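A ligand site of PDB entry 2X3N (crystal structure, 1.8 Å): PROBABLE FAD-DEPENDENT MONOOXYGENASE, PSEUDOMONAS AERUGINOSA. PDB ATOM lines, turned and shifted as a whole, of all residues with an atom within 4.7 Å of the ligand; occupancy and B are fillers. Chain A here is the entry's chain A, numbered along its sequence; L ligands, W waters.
Water W4 lies within hydrogen-bond range of O of Ala 161 (2.6 Å), O14 of the ligand (2.7 Å), N of Gly 18 (2.8 Å) and N of Gly 15 (3.0 Å).
Water W2 bridges an oxygen (O2) of the ligand and the side-chain carboxylate (OD2) of Asp 293.
Water W1 bridges ND2 of Asn 12 (2.7 Å) and N4 of the ligand (2.8 Å).
Water W9 bridges an oxygen (O8) of the ligand (2.9 Å) and the backbone carbonyl oxygen of Pro 300 (3.0 Å).
Water W7 bridges the backbone carbonyl oxygen of Val 298 and an oxygen (O7) of the ligand.
O14 of the ligand lies within hydrogen-bond range of N of Gly 17.
The backbone NH of Gln 304 lies within hydrogen-bond range of an oxygen (O7) of the ligand.
The backbone NH of Gln 37 is in hydrogen-bond range of a nitrogen (N5) of the ligand, at 3.2 Å.
The backbone NH (N) of Asp 293 is in hydrogen-bond range of an oxygen (O13) of the ligand (2.9 Å).
An oxygen (O9) of the ligand lies within hydrogen-bond range of the backbone NH of Ala 47 (3.0 Å).
The side-chain amide oxygen (OE1) of Gln 37 sits close to a nitrogen (N2) of the ligand, 3.2 Å away.
O10 of the ligand is in hydrogen-bond range of OD2 of Asp 293, 2.8 Å away.
The backbone NH (N) of Gly 305 sits at hydrogen-bond distance from an oxygen (O7) of the ligand (2.9 Å).
The backbone carbonyl oxygen (O) of Pro 300 is in hydrogen-bond range of a nitrogen (N7) of the ligand.
O6 of the ligand is in hydrogen-bond range of OE2 of Glu 36 (2.6 Å).
Merely in contact with the ligand: Asp 162, Gly 303, Gly 15, Gly 292, Gly 13, Gly 46, Gly 272, Ile 273, Ala 161, Tyr 167, Asn 45, Pro 274, Ala 309, Ile 16, Asn 12, Gly 163, Val 35, Cys 14 and Met 306.
Hydrophobic or aromatic side chains within 4 Å of the ligand: Ile 16, Ala 47, Tyr 167, Ile 273, Pro 274, Pro 300 and Ala 309.
Within 4 Å of the ligand: Asn 12, Gly 13, Cys 14, Gly 15, Ile 16, Gly 17, Val 35, Glu 36, Gln 37, Asn 45, Gly 46, Ala 47, Ala 161, Asp 162, Gly 163, Tyr 167, Gly 272, Ile 273, Pro 274, Gly 292, Asp 293, Pro 300, Gly 303, Gln 304, Gly 305, Met 306 and Ala 309.
Along chain A the residues within 4 Å of the ligand span positions 12 to 309.
The side-chain carboxylate (OE1) of Glu 36 is in hydrogen-bond range of the backbone NH (N) of Cys 14 (2.8 Å).
N of Gln 304 sits close to OG1 of Thr 302, at 3.2 Å.
N of Gln 37 sits at hydrogen-bond distance from O of Thr 129 (3.3 Å).
N of Ala 161 is in hydrogen-bond range of O of Asn 12, 2.8 Å away.
The backbone NH of Cys 106 lies within hydrogen-bond range of the backbone carbonyl oxygen of Ala 47 (3.0 Å).
OD2 of Asp 162 is in hydrogen-bond range of N of Tyr 167 (3.1 Å).
The backbone NH (N) of Thr 129 is in hydrogen-bond range of the backbone carbonyl oxygen (O) of Glu 36 (3.0 Å).
The side-chain amide oxygen of Asn 12 lies close to the side-chain carboxylate of Asp 162 (2.8 Å).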
ATOM      1  N   ASN A  12       8.768 -25.737 -22.423  1.00  0.00           N
ATOM      2  CA  ASN A  12       8.542 -25.613 -20.993  1.00  0.00           C
ATOM      3  C   ASN A  12       7.051 -25.550 -20.696  1.00  0.00           C
ATOM      4  O   ASN A  12       6.399 -24.559 -21.047  1.00  0.00           O
ATOM      5  CB  ASN A  12       9.261 -24.361 -20.429  1.00  0.00           C
ATOM      6  CG  ASN A  12       9.566 -24.472 -18.948  1.00  0.00           C
ATOM      7  OD1 ASN A  12       9.274 -23.541 -18.162  1.00  0.00           O
ATOM      8  ND2 ASN A  12      10.162 -25.581 -18.552  1.00  0.00           N
ATOM      9  N   GLY A  13       6.525 -26.605 -20.084  1.00  0.00           N
ATOM     10  CA  GLY A  13       5.124 -26.646 -19.673  1.00  0.00           C
ATOM     11  C   GLY A  13       4.363 -27.594 -20.582  1.00  0.00           C
ATOM     12  O   GLY A  13       4.447 -27.483 -21.804  1.00  0.00           O
ATOM     13  N   CYS A  14       3.641 -28.532 -19.971  1.00  0.00           N
ATOM     14  CA  CYS A  14       2.821 -29.480 -20.710  1.00  0.00           C
ATOM     15  C   CYS A  14       1.347 -29.272 -20.363  1.00  0.00           C
ATOM     16  O   CYS A  14       0.599 -30.220 -20.071  1.00  0.00           O
ATOM     17  CB  CYS A  14       3.286 -30.918 -20.428  1.00  0.00           C
ATOM     18  SG  CYS A  14       2.657 -32.107 -21.625  1.00  0.00           S
ATOM     19  N   GLY A  15       0.916 -28.013 -20.397  1.00  0.00           N
ATOM     20  CA  GLY A  15      -0.502 -27.720 -20.305  1.00  0.00           C
ATOM     21  C   GLY A  15      -1.142 -27.982 -21.657  1.00  0.00           C
ATOM     22  O   GLY A  15      -0.538 -28.612 -22.544  1.00  0.00           O
ATOM     23  N   ILE A  16      -2.348 -27.459 -21.852  1.00  0.00           N
ATOM     24  CA  ILE A  16      -3.042 -27.720 -23.135  1.00  0.00           C
ATOM     25  C   ILE A  16      -2.263 -27.160 -24.349  1.00  0.00           C
ATOM     26  O   ILE A  16      -2.150 -27.839 -25.377  1.00  0.00           O
ATOM     27  CB  ILE A  16      -4.511 -27.276 -23.136  1.00  0.00           C
ATOM     28  CG1 ILE A  16      -5.232 -27.772 -24.402  1.00  0.00           C
ATOM     29  CG2 ILE A  16      -4.660 -25.747 -22.993  1.00  0.00           C
ATOM     30  CD1 ILE A  16      -5.214 -29.328 -24.546  1.00  0.00           C
ATOM     31  N   GLY A  17      -1.718 -25.945 -24.204  1.00  0.00           N
ATOM     32  CA  GLY A  17      -0.937 -25.330 -25.280  1.00  0.00           C
ATOM     33  C   GLY A  17       0.343 -26.095 -25.598  1.00  0.00           C
ATOM     34  O   GLY A  17       0.632 -26.397 -26.784  1.00  0.00           O
ATOM     35  N   GLY A  18       1.104 -26.419 -24.543  1.00  0.00           N
ATOM     36  CA  GLY A  18       2.374 -27.133 -24.669  1.00  0.00           C
ATOM     37  C   GLY A  18       2.179 -28.517 -25.248  1.00  0.00           C
ATOM     38  O   GLY A  18       2.941 -28.936 -26.140  1.00  0.00           O
ATOM     39  N   VAL A  35       9.034 -30.381 -20.772  1.00  0.00           N
ATOM     40  CA  VAL A  35       9.399 -30.341 -19.369  1.00  0.00           C
ATOM     41  C   VAL A  35       8.194 -29.835 -18.602  1.00  0.00           C
ATOM     42  O   VAL A  35       7.706 -28.727 -18.872  1.00  0.00           O
ATOM     43  CB  VAL A  35      10.622 -29.423 -19.150  1.00  0.00           C
ATOM     44  CG1 VAL A  35      10.929 -29.234 -17.687  1.00  0.00           C
ATOM     45  CG2 VAL A  35      11.826 -29.993 -19.872  1.00  0.00           C
ATOM     46  N   GLU A  36       7.701 -30.640 -17.666  1.00  0.00           N
ATOM     47  CA  GLU A  36       6.523 -30.283 -16.884  1.00  0.00           C
ATOM     48  C   GLU A  36       6.798 -30.481 -15.394  1.00  0.00           C
ATOM     49  O   GLU A  36       7.224 -31.559 -14.976  1.00  0.00           O
ATOM     50  CB  GLU A  36       5.307 -31.094 -17.344  1.00  0.00           C
ATOM     51  CG  GLU A  36       4.068 -31.049 -16.403  1.00  0.00           C
ATOM     52  CD  GLU A  36       3.474 -29.659 -16.260  1.00  0.00           C
ATOM     53  OE1 GLU A  36       3.121 -29.060 -17.287  1.00  0.00           O
ATOM     54  OE2 GLU A  36       3.352 -29.164 -15.118  1.00  0.00           O
ATOM     55  N   GLN A  37       6.560 -29.434 -14.603  1.00  0.00           N
ATOM     56  CA  GLN A  37       6.873 -29.467 -13.158  1.00  0.00           C
ATOM     57  C   GLN A  37       5.965 -30.410 -12.368  1.00  0.00           C
ATOM     58  O   GLN A  37       6.381 -30.975 -11.341  1.00  0.00           O
ATOM     59  CB  GLN A  37       6.824 -28.038 -12.567  1.00  0.00           C
ATOM     60  CG  GLN A  37       5.427 -27.395 -12.530  1.00  0.00           C
ATOM     61  CD  GLN A  37       5.427 -25.883 -12.174  1.00  0.00           C
ATOM     62  OE1 GLN A  37       4.415 -25.200 -12.334  1.00  0.00           O
ATOM     63  NE2 GLN A  37       6.544 -25.389 -11.672  1.00  0.00           N
ATOM     64  N   ALA A  38       4.729 -30.575 -12.832  1.00  0.00           N
ATOM     65  CA  ALA A  38       3.733 -31.381 -12.129  1.00  0.00           C
ATOM     66  C   ALA A  38       3.816 -32.840 -12.581  1.00  0.00           C
ATOM     67  O   ALA A  38       4.470 -33.140 -13.586  1.00  0.00           O
ATOM     68  CB  ALA A  38       2.338 -30.813 -12.381  1.00  0.00           C
ATOM     69  N   ASN A  45      -8.270 -28.668 -13.786  1.00  0.00           N
ATOM     70  CA  ASN A  45      -9.417 -27.801 -14.010  1.00  0.00           C
ATOM     71  C   ASN A  45      -8.974 -26.576 -14.801  1.00  0.00           C
ATOM     72  O   ASN A  45      -7.930 -25.972 -14.488  1.00  0.00           O
ATOM     73  CB  ASN A  45     -10.035 -27.346 -12.685  1.00  0.00           C
ATOM     74  CG  ASN A  45     -10.343 -28.519 -11.744  1.00  0.00           C
ATOM     75  OD1 ASN A  45     -11.514 -28.837 -11.500  1.00  0.00           O
ATOM     76  ND2 ASN A  45      -9.291 -29.142 -11.197  1.00  0.00           N
ATOM     77  N   GLY A  46      -9.732 -26.217 -15.819  1.00  0.00           N
ATOM     78  CA  GLY A  46      -9.382 -25.092 -16.682  1.00  0.00           C
ATOM     79  C   GLY A  46     -10.547 -24.739 -17.561  1.00  0.00           C
ATOM     80  O   GLY A  46     -11.692 -25.101 -17.257  1.00  0.00           O
ATOM     81  N   ALA A  47     -10.271 -24.061 -18.661  1.00  0.00           N
ATOM     82  CA  ALA A  47     -11.327 -23.613 -19.571  1.00  0.00           C
ATOM     83  C   ALA A  47     -12.012 -24.799 -20.244  1.00  0.00           C
ATOM     84  O   ALA A  47     -11.452 -25.912 -20.278  1.00  0.00           O
ATOM     85  CB  ALA A  47     -10.757 -22.650 -20.597  1.00  0.00           C
ATOM     86  N   CYS A 106     -10.854 -28.843 -20.413  1.00  0.00           N
ATOM     87  CA  CYS A 106      -9.425 -28.737 -20.701  1.00  0.00           C
ATOM     88  C   CYS A 106      -8.709 -30.046 -20.371  1.00  0.00           C
ATOM     89  O   CYS A 106      -7.988 -30.587 -21.199  1.00  0.00           O
ATOM     90  CB  CYS A 106      -8.794 -27.602 -19.885  1.00  0.00           C
ATOM     91  SG  CYS A 106      -7.063 -27.339 -20.407  1.00  0.00           S
ATOM     92  N   THR A 129       9.682 -32.335 -13.536  1.00  0.00           N
ATOM     93  CA  THR A 129      10.991 -31.901 -13.989  1.00  0.00           C
ATOM     94  C   THR A 129      10.919 -30.409 -14.258  1.00  0.00           C
ATOM     95  O   THR A 129       9.871 -29.891 -14.627  1.00  0.00           O
ATOM     96  CB  THR A 129      11.408 -32.657 -15.257  1.00  0.00           C
ATOM     97  OG1 THR A 129      11.404 -34.060 -14.982  1.00  0.00           O
ATOM     98  CG2 THR A 129      12.815 -32.261 -15.731  1.00  0.00           C
ATOM     99  N   ARG A 130      12.033 -29.704 -14.072  1.00  0.00           N
ATOM    100  CA  ARG A 130      12.102 -28.276 -14.357  1.00  0.00           C
ATOM    101  C   ARG A 130      13.472 -27.873 -14.908  1.00  0.00           C
ATOM    102  O   ARG A 130      14.472 -28.571 -14.724  1.00  0.00           O
ATOM    103  CB  ARG A 130      11.753 -27.430 -13.124  1.00  0.00           C
ATOM    104  CG  ARG A 130      12.469 -27.824 -11.846  1.00  0.00           C
ATOM    105  CD  ARG A 130      12.026 -26.981 -10.660  1.00  0.00           C
ATOM    106  NE  ARG A 130      10.716 -27.373 -10.119  1.00  0.00           N
ATOM    107  CZ  ARG A 130       9.578 -26.706 -10.291  1.00  0.00           C
ATOM    108  NH1 ARG A 130       9.552 -25.584 -11.011  1.00  0.00           N
ATOM    109  NH2 ARG A 130       8.456 -27.154  -9.723  1.00  0.00           N
ATOM    110  N   ALA A 161       5.519 -22.484 -22.784  1.00  0.00           N
ATOM    111  CA  ALA A 161       4.109 -22.927 -22.773  1.00  0.00           C
ATOM    112  C   ALA A 161       3.732 -23.128 -21.302  1.00  0.00           C
ATOM    113  O   ALA A 161       2.966 -24.030 -20.939  1.00  0.00           O
ATOM    114  CB  ALA A 161       3.978 -24.234 -23.578  1.00  0.00           C
ATOM    115  N   ASP A 162       4.278 -22.241 -20.460  1.00  0.00           N
ATOM    116  CA  ASP A 162       4.276 -22.470 -19.019  1.00  0.00           C
ATOM    117  C   ASP A 162       3.332 -21.543 -18.253  1.00  0.00           C
ATOM    118  O   ASP A 162       3.482 -21.362 -17.041  1.00  0.00           O
ATOM    119  CB  ASP A 162       5.706 -22.456 -18.443  1.00  0.00           C
ATOM    120  CG  ASP A 162       6.572 -21.324 -18.985  1.00  0.00           C
ATOM    121  OD1 ASP A 162       6.134 -20.511 -19.831  1.00  0.00           O
ATOM    122  OD2 ASP A 162       7.743 -21.259 -18.556  1.00  0.00           O
ATOM    123  N   GLY A 163       2.368 -20.973 -18.981  1.00  0.00           N
ATOM    124  CA  GLY A 163       1.163 -20.435 -18.337  1.00  0.00           C
ATOM    125  C   GLY A 163       1.302 -19.030 -17.781  1.00  0.00           C
ATOM    126  O   GLY A 163       2.266 -18.309 -18.081  1.00  0.00           O
ATOM    127  N   TYR A 167       7.747 -19.084 -16.297  1.00  0.00           N
ATOM    128  CA  TYR A 167       9.184 -19.058 -15.985  1.00  0.00           C
ATOM    129  C   TYR A 167       9.979 -18.535 -17.190  1.00  0.00           C
ATOM    130  O   TYR A 167      10.923 -17.787 -17.022  1.00  0.00           O
ATOM    131  CB  TYR A 167       9.659 -20.481 -15.675  1.00  0.00           C
ATOM    132  CG  TYR A 167      11.152 -20.648 -15.541  1.00  0.00           C
ATOM    133  CD1 TYR A 167      11.788 -20.430 -14.318  1.00  0.00           C
ATOM    134  CD2 TYR A 167      11.926 -21.042 -16.629  1.00  0.00           C
ATOM    135  CE1 TYR A 167      13.161 -20.601 -14.198  1.00  0.00           C
ATOM    136  CE2 TYR A 167      13.285 -21.207 -16.517  1.00  0.00           C
ATOM    137  CZ  TYR A 167      13.896 -20.988 -15.310  1.00  0.00           C
ATOM    138  OH  TYR A 167      15.256 -21.164 -15.218  1.00  0.00           O
ATOM    139  N   VAL A 188     -16.045 -21.047 -10.490  1.00  0.00           N
ATOM    140  CA  VAL A 188     -16.743 -22.068 -11.253  1.00  0.00           C
ATOM    141  C   VAL A 188     -16.975 -23.308 -10.399  1.00  0.00           C
ATOM    142  O   VAL A 188     -16.080 -23.766  -9.699  1.00  0.00           O
ATOM    143  CB  VAL A 188     -15.992 -22.419 -12.582  1.00  0.00           C
ATOM    144  CG1 VAL A 188     -14.553 -22.905 -12.331  1.00  0.00           C
ATOM    145  CG2 VAL A 188     -16.814 -23.454 -13.407  1.00  0.00           C
ATOM    146  N   LYS A 271     -14.449 -23.184  -7.433  1.00  0.00           N
ATOM    147  CA  LYS A 271     -13.039 -22.860  -7.590  1.00  0.00           C
ATOM    148  C   LYS A 271     -12.925 -21.460  -8.194  1.00  0.00           C
ATOM    149  O   LYS A 271     -13.684 -21.101  -9.089  1.00  0.00           O
ATOM    150  CB  LYS A 271     -12.335 -23.859  -8.530  1.00  0.00           C
ATOM    151  CG  LYS A 271     -12.713 -25.340  -8.340  1.00  0.00           C
ATOM    152  CD  LYS A 271     -12.278 -25.896  -6.972  1.00  0.00           C
ATOM    153  CE  LYS A 271     -12.643 -27.384  -6.854  1.00  0.00           C
ATOM    154  NZ  LYS A 271     -12.495 -27.845  -5.431  1.00  0.00           N
ATOM    155  N   GLY A 272     -11.970 -20.685  -7.696  1.00  0.00           N
ATOM    156  CA  GLY A 272     -11.618 -19.418  -8.345  1.00  0.00           C
ATOM    157  C   GLY A 272     -11.038 -19.632  -9.740  1.00  0.00           C
ATOM    158  O   GLY A 272     -10.462 -20.676 -10.043  1.00  0.00           O
ATOM    159  N   ILE A 273     -11.189 -18.634 -10.586  1.00  0.00           N
ATOM    160  CA  ILE A 273     -10.601 -18.640 -11.913  1.00  0.00           C
ATOM    161  C   ILE A 273      -9.634 -17.478 -12.026  1.00  0.00           C
ATOM    162  O   ILE A 273      -9.973 -16.364 -11.629  1.00  0.00           O
ATOM    163  CB  ILE A 273     -11.706 -18.458 -13.012  1.00  0.00           C
ATOM    164  CG1 ILE A 273     -12.807 -19.510 -12.866  1.00  0.00           C
ATOM    165  CG2 ILE A 273     -11.065 -18.466 -14.417  1.00  0.00           C
ATOM    166  CD1 ILE A 273     -13.988 -19.314 -13.875  1.00  0.00           C
ATOM    167  N   PRO A 274      -8.440 -17.699 -12.585  1.00  0.00           N
ATOM    168  CA  PRO A 274      -7.526 -16.558 -12.680  1.00  0.00           C
ATOM    169  C   PRO A 274      -8.042 -15.453 -13.592  1.00  0.00           C
ATOM    170  O   PRO A 274      -8.638 -15.729 -14.635  1.00  0.00           O
ATOM    171  CB  PRO A 274      -6.248 -17.164 -13.299  1.00  0.00           C
ATOM    172  CG  PRO A 274      -6.362 -18.588 -13.149  1.00  0.00           C
ATOM    173  CD  PRO A 274      -7.821 -18.953 -13.054  1.00  0.00           C
ATOM    174  N   LEU A 291       3.699 -19.063 -25.936  1.00  0.00           N
ATOM    175  CA  LEU A 291       2.340 -19.264 -26.370  1.00  0.00           C
ATOM    176  C   LEU A 291       1.385 -19.206 -25.187  1.00  0.00           C
ATOM    177  O   LEU A 291       1.809 -19.338 -24.025  1.00  0.00           O
ATOM    178  CB  LEU A 291       2.183 -20.591 -27.120  1.00  0.00           C
ATOM    179  CG  LEU A 291       2.428 -21.896 -26.350  1.00  0.00           C
ATOM    180  CD1 LEU A 291       1.171 -22.309 -25.532  1.00  0.00           C
ATOM    181  CD2 LEU A 291       2.768 -23.034 -27.332  1.00  0.00           C
ATOM    182  N   GLY A 292       0.102 -19.034 -25.482  1.00  0.00           N
ATOM    183  CA  GLY A 292      -0.946 -19.173 -24.467  1.00  0.00           C
ATOM    184  C   GLY A 292      -0.868 -18.142 -23.365  1.00  0.00           C
ATOM    185  O   GLY A 292      -0.643 -16.965 -23.617  1.00  0.00           O
ATOM    186  N   ASP A 293      -1.073 -18.579 -22.127  1.00  0.00           N
ATOM    187  CA  ASP A 293      -1.156 -17.652 -20.996  1.00  0.00           C
ATOM    188  C   ASP A 293       0.200 -16.960 -20.692  1.00  0.00           C
ATOM    189  O   ASP A 293       0.238 -16.000 -19.934  1.00  0.00           O
ATOM    190  CB  ASP A 293      -1.688 -18.363 -19.747  1.00  0.00           C
ATOM    191  CG  ASP A 293      -3.212 -18.507 -19.737  1.00  0.00           C
ATOM    192  OD1 ASP A 293      -3.887 -18.053 -20.690  1.00  0.00           O
ATOM    193  OD2 ASP A 293      -3.730 -19.054 -18.752  1.00  0.00           O
ATOM    194  N   VAL A 298      -6.688 -13.366 -21.117  1.00  0.00           N
ATOM    195  CA  VAL A 298      -7.982 -12.813 -21.453  1.00  0.00           C
ATOM    196  C   VAL A 298      -8.952 -12.975 -20.276  1.00  0.00           C
ATOM    197  O   VAL A 298      -8.864 -13.934 -19.524  1.00  0.00           O
ATOM    198  CB  VAL A 298      -8.603 -13.464 -22.734  1.00  0.00           C
ATOM    199  CG1 VAL A 298      -7.726 -13.177 -23.926  1.00  0.00           C
ATOM    200  CG2 VAL A 298      -8.831 -14.974 -22.553  1.00  0.00           C
ATOM    201  N   HIS A 299      -9.854 -12.013 -20.104  1.00  0.00           N
ATOM    202  CA  HIS A 299     -10.835 -12.201 -19.055  1.00  0.00           C
ATOM    203  C   HIS A 299     -11.599 -13.522 -19.265  1.00  0.00           C
ATOM    204  O   HIS A 299     -12.075 -13.806 -20.395  1.00  0.00           O
ATOM    205  CB  HIS A 299     -11.759 -10.969 -18.916  1.00  0.00           C
ATOM    206  CG  HIS A 299     -12.556 -10.979 -17.651  1.00  0.00           C
ATOM    207  ND1 HIS A 299     -12.326 -10.115 -16.611  1.00  0.00           N
ATOM    208  CD2 HIS A 299     -13.540 -11.803 -17.251  1.00  0.00           C
ATOM    209  CE1 HIS A 299     -13.152 -10.394 -15.619  1.00  0.00           C
ATOM    210  NE2 HIS A 299     -13.892 -11.418 -15.981  1.00  0.00           N
ATOM    211  N   PRO A 300     -11.684 -14.353 -18.213  1.00  0.00           N
ATOM    212  CA  PRO A 300     -12.378 -15.625 -18.344  1.00  0.00           C
ATOM    213  C   PRO A 300     -13.861 -15.520 -18.758  1.00  0.00           C
ATOM    214  O   PRO A 300     -14.456 -16.510 -19.143  1.00  0.00           O
ATOM    215  CB  PRO A 300     -12.204 -16.291 -16.974  1.00  0.00           C
ATOM    216  CG  PRO A 300     -11.930 -15.153 -16.017  1.00  0.00           C
ATOM    217  CD  PRO A 300     -11.170 -14.149 -16.840  1.00  0.00           C
ATOM    218  N   THR A 302     -14.781 -14.407 -21.395  1.00  0.00           N
ATOM    219  CA  THR A 302     -14.738 -14.762 -22.827  1.00  0.00           C
ATOM    220  C   THR A 302     -14.748 -16.265 -23.021  1.00  0.00           C
ATOM    221  O   THR A 302     -15.110 -16.763 -24.084  1.00  0.00           O
ATOM    222  CB  THR A 302     -13.489 -14.202 -23.551  1.00  0.00           C
ATOM    223  OG1 THR A 302     -12.311 -14.873 -23.081  1.00  0.00           O
ATOM    224  CG2 THR A 302     -13.334 -12.686 -23.369  1.00  0.00           C
ATOM    225  N   GLY A 303     -14.312 -17.004 -22.007  1.00  0.00           N
ATOM    226  CA  GLY A 303     -14.180 -18.463 -22.092  1.00  0.00           C
ATOM    227  C   GLY A 303     -12.996 -18.967 -22.916  1.00  0.00           C
ATOM    228  O   GLY A 303     -12.787 -20.173 -22.996  1.00  0.00           O
ATOM    229  N   GLN A 304     -12.196 -18.064 -23.466  1.00  0.00           N
ATOM    230  CA  GLN A 304     -11.216 -18.412 -24.514  1.00  0.00           C
ATOM    231  C   GLN A 304      -9.772 -18.736 -24.122  1.00  0.00           C
ATOM    232  O   GLN A 304      -8.934 -18.933 -25.017  1.00  0.00           O
ATOM    233  CB  GLN A 304     -11.236 -17.344 -25.586  1.00  0.00           C
ATOM    234  CG  GLN A 304     -12.530 -17.361 -26.394  1.00  0.00           C
ATOM    235  CD  GLN A 304     -12.372 -16.772 -27.766  1.00  0.00           C
ATOM    236  OE1 GLN A 304     -13.241 -16.025 -28.223  1.00  0.00           O
ATOM    237  NE2 GLN A 304     -11.269 -17.081 -28.429  1.00  0.00           N
ATOM    238  N   GLY A 305      -9.472 -18.850 -22.812  1.00  0.00           N
ATOM    239  CA  GLY A 305      -8.107 -19.204 -22.376  1.00  0.00           C
ATOM    240  C   GLY A 305      -7.477 -20.433 -23.050  1.00  0.00           C
ATOM    241  O   GLY A 305      -6.340 -20.376 -23.577  1.00  0.00           O
ATOM    242  N   MET A 306      -8.204 -21.557 -23.033  1.00  0.00           N
ATOM    243  CA  MET A 306      -7.743 -22.776 -23.725  1.00  0.00           C
ATOM    244  C   MET A 306      -7.742 -22.569 -25.224  1.00  0.00           C
ATOM    245  O   MET A 306      -6.744 -22.918 -25.900  1.00  0.00           O
ATOM    246  CB  MET A 306      -8.580 -24.004 -23.363  1.00  0.00           C
ATOM    247  CG  MET A 306      -8.368 -25.191 -24.314  1.00  0.00           C
ATOM    248  SD  MET A 306      -9.205 -26.687 -23.785  1.00  0.00           S
ATOM    249  CE  MET A 306     -10.920 -26.111 -23.720  1.00  0.00           C
ATOM    250  N   ALA A 309      -4.737 -20.601 -26.490  1.00  0.00           N
ATOM    251  CA  ALA A 309      -3.513 -21.417 -26.341  1.00  0.00           C
ATOM    252  C   ALA A 309      -3.398 -22.428 -27.472  1.00  0.00           C
ATOM    253  O   ALA A 309      -2.309 -22.603 -28.039  1.00  0.00           O
ATOM    254  CB  ALA A 309      -3.473 -22.101 -24.972  1.00  0.00           C
HETATM  255  P1  LIG L   1      -1.653 -23.795 -18.705  1.00  0.00           P
HETATM  256  O1  LIG L   1      -2.927 -24.659 -19.112  1.00  0.00           O
HETATM  257  O2  LIG L   1      -1.703 -22.983 -17.441  1.00  0.00           O
HETATM  258  O3  LIG L   1      -0.425 -24.813 -18.737  1.00  0.00           O
HETATM  259  C1  LIG L   1       0.854 -24.407 -18.172  1.00  0.00           C
HETATM  260  C2  LIG L   1       1.645 -25.644 -17.816  1.00  0.00           C
HETATM  261  O4  LIG L   1       2.978 -25.218 -17.472  1.00  0.00           O
HETATM  262  C3  LIG L   1       1.049 -26.294 -16.551  1.00  0.00           C
HETATM  263  O5  LIG L   1       0.966 -27.708 -16.780  1.00  0.00           O
HETATM  264  C4  LIG L   1       2.074 -25.961 -15.460  1.00  0.00           C
HETATM  265  O6  LIG L   1       2.145 -27.000 -14.469  1.00  0.00           O
HETATM  266  C5  LIG L   1       3.355 -25.925 -16.280  1.00  0.00           C
HETATM  267  N1  LIG L   1       4.421 -25.065 -15.701  1.00  0.00           N
HETATM  268  C6  LIG L   1       4.277 -23.822 -15.198  1.00  0.00           C
HETATM  269  N2  LIG L   1       5.483 -23.401 -14.785  1.00  0.00           N
HETATM  270  C7  LIG L   1       6.379 -24.355 -15.047  1.00  0.00           C
HETATM  271  C8  LIG L   1       7.766 -24.477 -14.861  1.00  0.00           C
HETATM  272  N3  LIG L   1       8.475 -23.486 -14.300  1.00  0.00           N
HETATM  273  N4  LIG L   1       8.369 -25.597 -15.244  1.00  0.00           N
HETATM  274  C9  LIG L   1       7.682 -26.591 -15.807  1.00  0.00           C
HETATM  275  N5  LIG L   1       6.366 -26.517 -16.001  1.00  0.00           N
HETATM  276  C10 LIG L   1       5.700 -25.410 -15.638  1.00  0.00           C
HETATM  277  N6  LIG L   1     -10.110 -19.333 -19.022  1.00  0.00           N
HETATM  278  C11 LIG L   1     -11.193 -18.701 -19.604  1.00  0.00           C
HETATM  279  O7  LIG L   1     -11.010 -17.929 -20.525  1.00  0.00           O
HETATM  280  N7  LIG L   1     -12.507 -18.944 -19.132  1.00  0.00           N
HETATM  281  C12 LIG L   1     -12.715 -19.810 -18.051  1.00  0.00           C
HETATM  282  O8  LIG L   1     -13.855 -20.020 -17.636  1.00  0.00           O
HETATM  283  C13 LIG L   1     -11.607 -20.455 -17.481  1.00  0.00           C
HETATM  284  N8  LIG L   1     -11.786 -21.353 -16.432  1.00  0.00           N
HETATM  285  C14 LIG L   1     -10.670 -21.704 -15.658  1.00  0.00           C
HETATM  286  C15 LIG L   1     -10.882 -22.304 -14.440  1.00  0.00           C
HETATM  287  C16 LIG L   1      -9.798 -22.646 -13.642  1.00  0.00           C
HETATM  288  C17 LIG L   1     -10.084 -23.305 -12.288  1.00  0.00           C
HETATM  289  C18 LIG L   1      -8.494 -22.363 -14.074  1.00  0.00           C
HETATM  290  C19 LIG L   1      -7.259 -22.732 -13.215  1.00  0.00           C
HETATM  291  C20 LIG L   1      -8.294 -21.768 -15.311  1.00  0.00           C
HETATM  292  C21 LIG L   1      -9.390 -21.431 -16.127  1.00  0.00           C
HETATM  293  N9  LIG L   1      -9.230 -20.787 -17.361  1.00  0.00           N
HETATM  294  C22 LIG L   1     -10.320 -20.200 -17.960  1.00  0.00           C
HETATM  295  C23 LIG L   1      -7.893 -20.514 -17.949  1.00  0.00           C
HETATM  296  C24 LIG L   1      -7.509 -21.518 -19.006  1.00  0.00           C
HETATM  297  O9  LIG L   1      -7.522 -22.793 -18.353  1.00  0.00           O
HETATM  298  C25 LIG L   1      -6.071 -21.173 -19.411  1.00  0.00           C
HETATM  299  O10 LIG L   1      -6.085 -19.918 -20.079  1.00  0.00           O
HETATM  300  C26 LIG L   1      -5.431 -22.217 -20.320  1.00  0.00           C
HETATM  301  O11 LIG L   1      -5.215 -23.469 -19.599  1.00  0.00           O
HETATM  302  C27 LIG L   1      -4.104 -21.680 -20.882  1.00  0.00           C
HETATM  303  O12 LIG L   1      -3.356 -22.757 -21.409  1.00  0.00           O
HETATM  304  P2  LIG L   1      -1.755 -22.755 -21.412  1.00  0.00           P
HETATM  305  O13 LIG L   1      -1.225 -21.441 -21.988  1.00  0.00           O
HETATM  306  O14 LIG L   1      -1.328 -23.987 -22.138  1.00  0.00           O
HETATM  307  O15 LIG L   1      -1.310 -22.759 -19.886  1.00  0.00           O
HETATM  308  O   HOH W   1      11.077 -25.475 -16.016  1.00  0.00           O
HETATM  309  O   HOH W   2      -2.025 -20.352 -16.973  1.00  0.00           O
HETATM  310  O   HOH W   3       1.433 -20.980 -21.742  1.00  0.00           O
HETATM  311  O   HOH W   4       0.928 -25.382 -21.928  1.00  0.00           O
HETATM  312  O   HOH W   5       7.856 -21.154 -12.368  1.00  0.00           O
HETATM  313  O   HOH W   6     -15.843 -21.023 -19.158  1.00  0.00           O
HETATM  314  O   HOH W   7      -8.633 -16.660 -19.376  1.00  0.00           O
HETATM  315  O   HOH W   8      -1.949 -28.525 -17.051  1.00  0.00           O
HETATM  316  O   HOH W   9     -16.327 -18.753 -18.475  1.00  0.00           O
HETATM  317  O   HOH W  10       0.316 -22.862 -14.869  1.00  0.00           O
HETATM  318  O   HOH W  11     -14.582 -22.014 -16.000  1.00  0.00           O
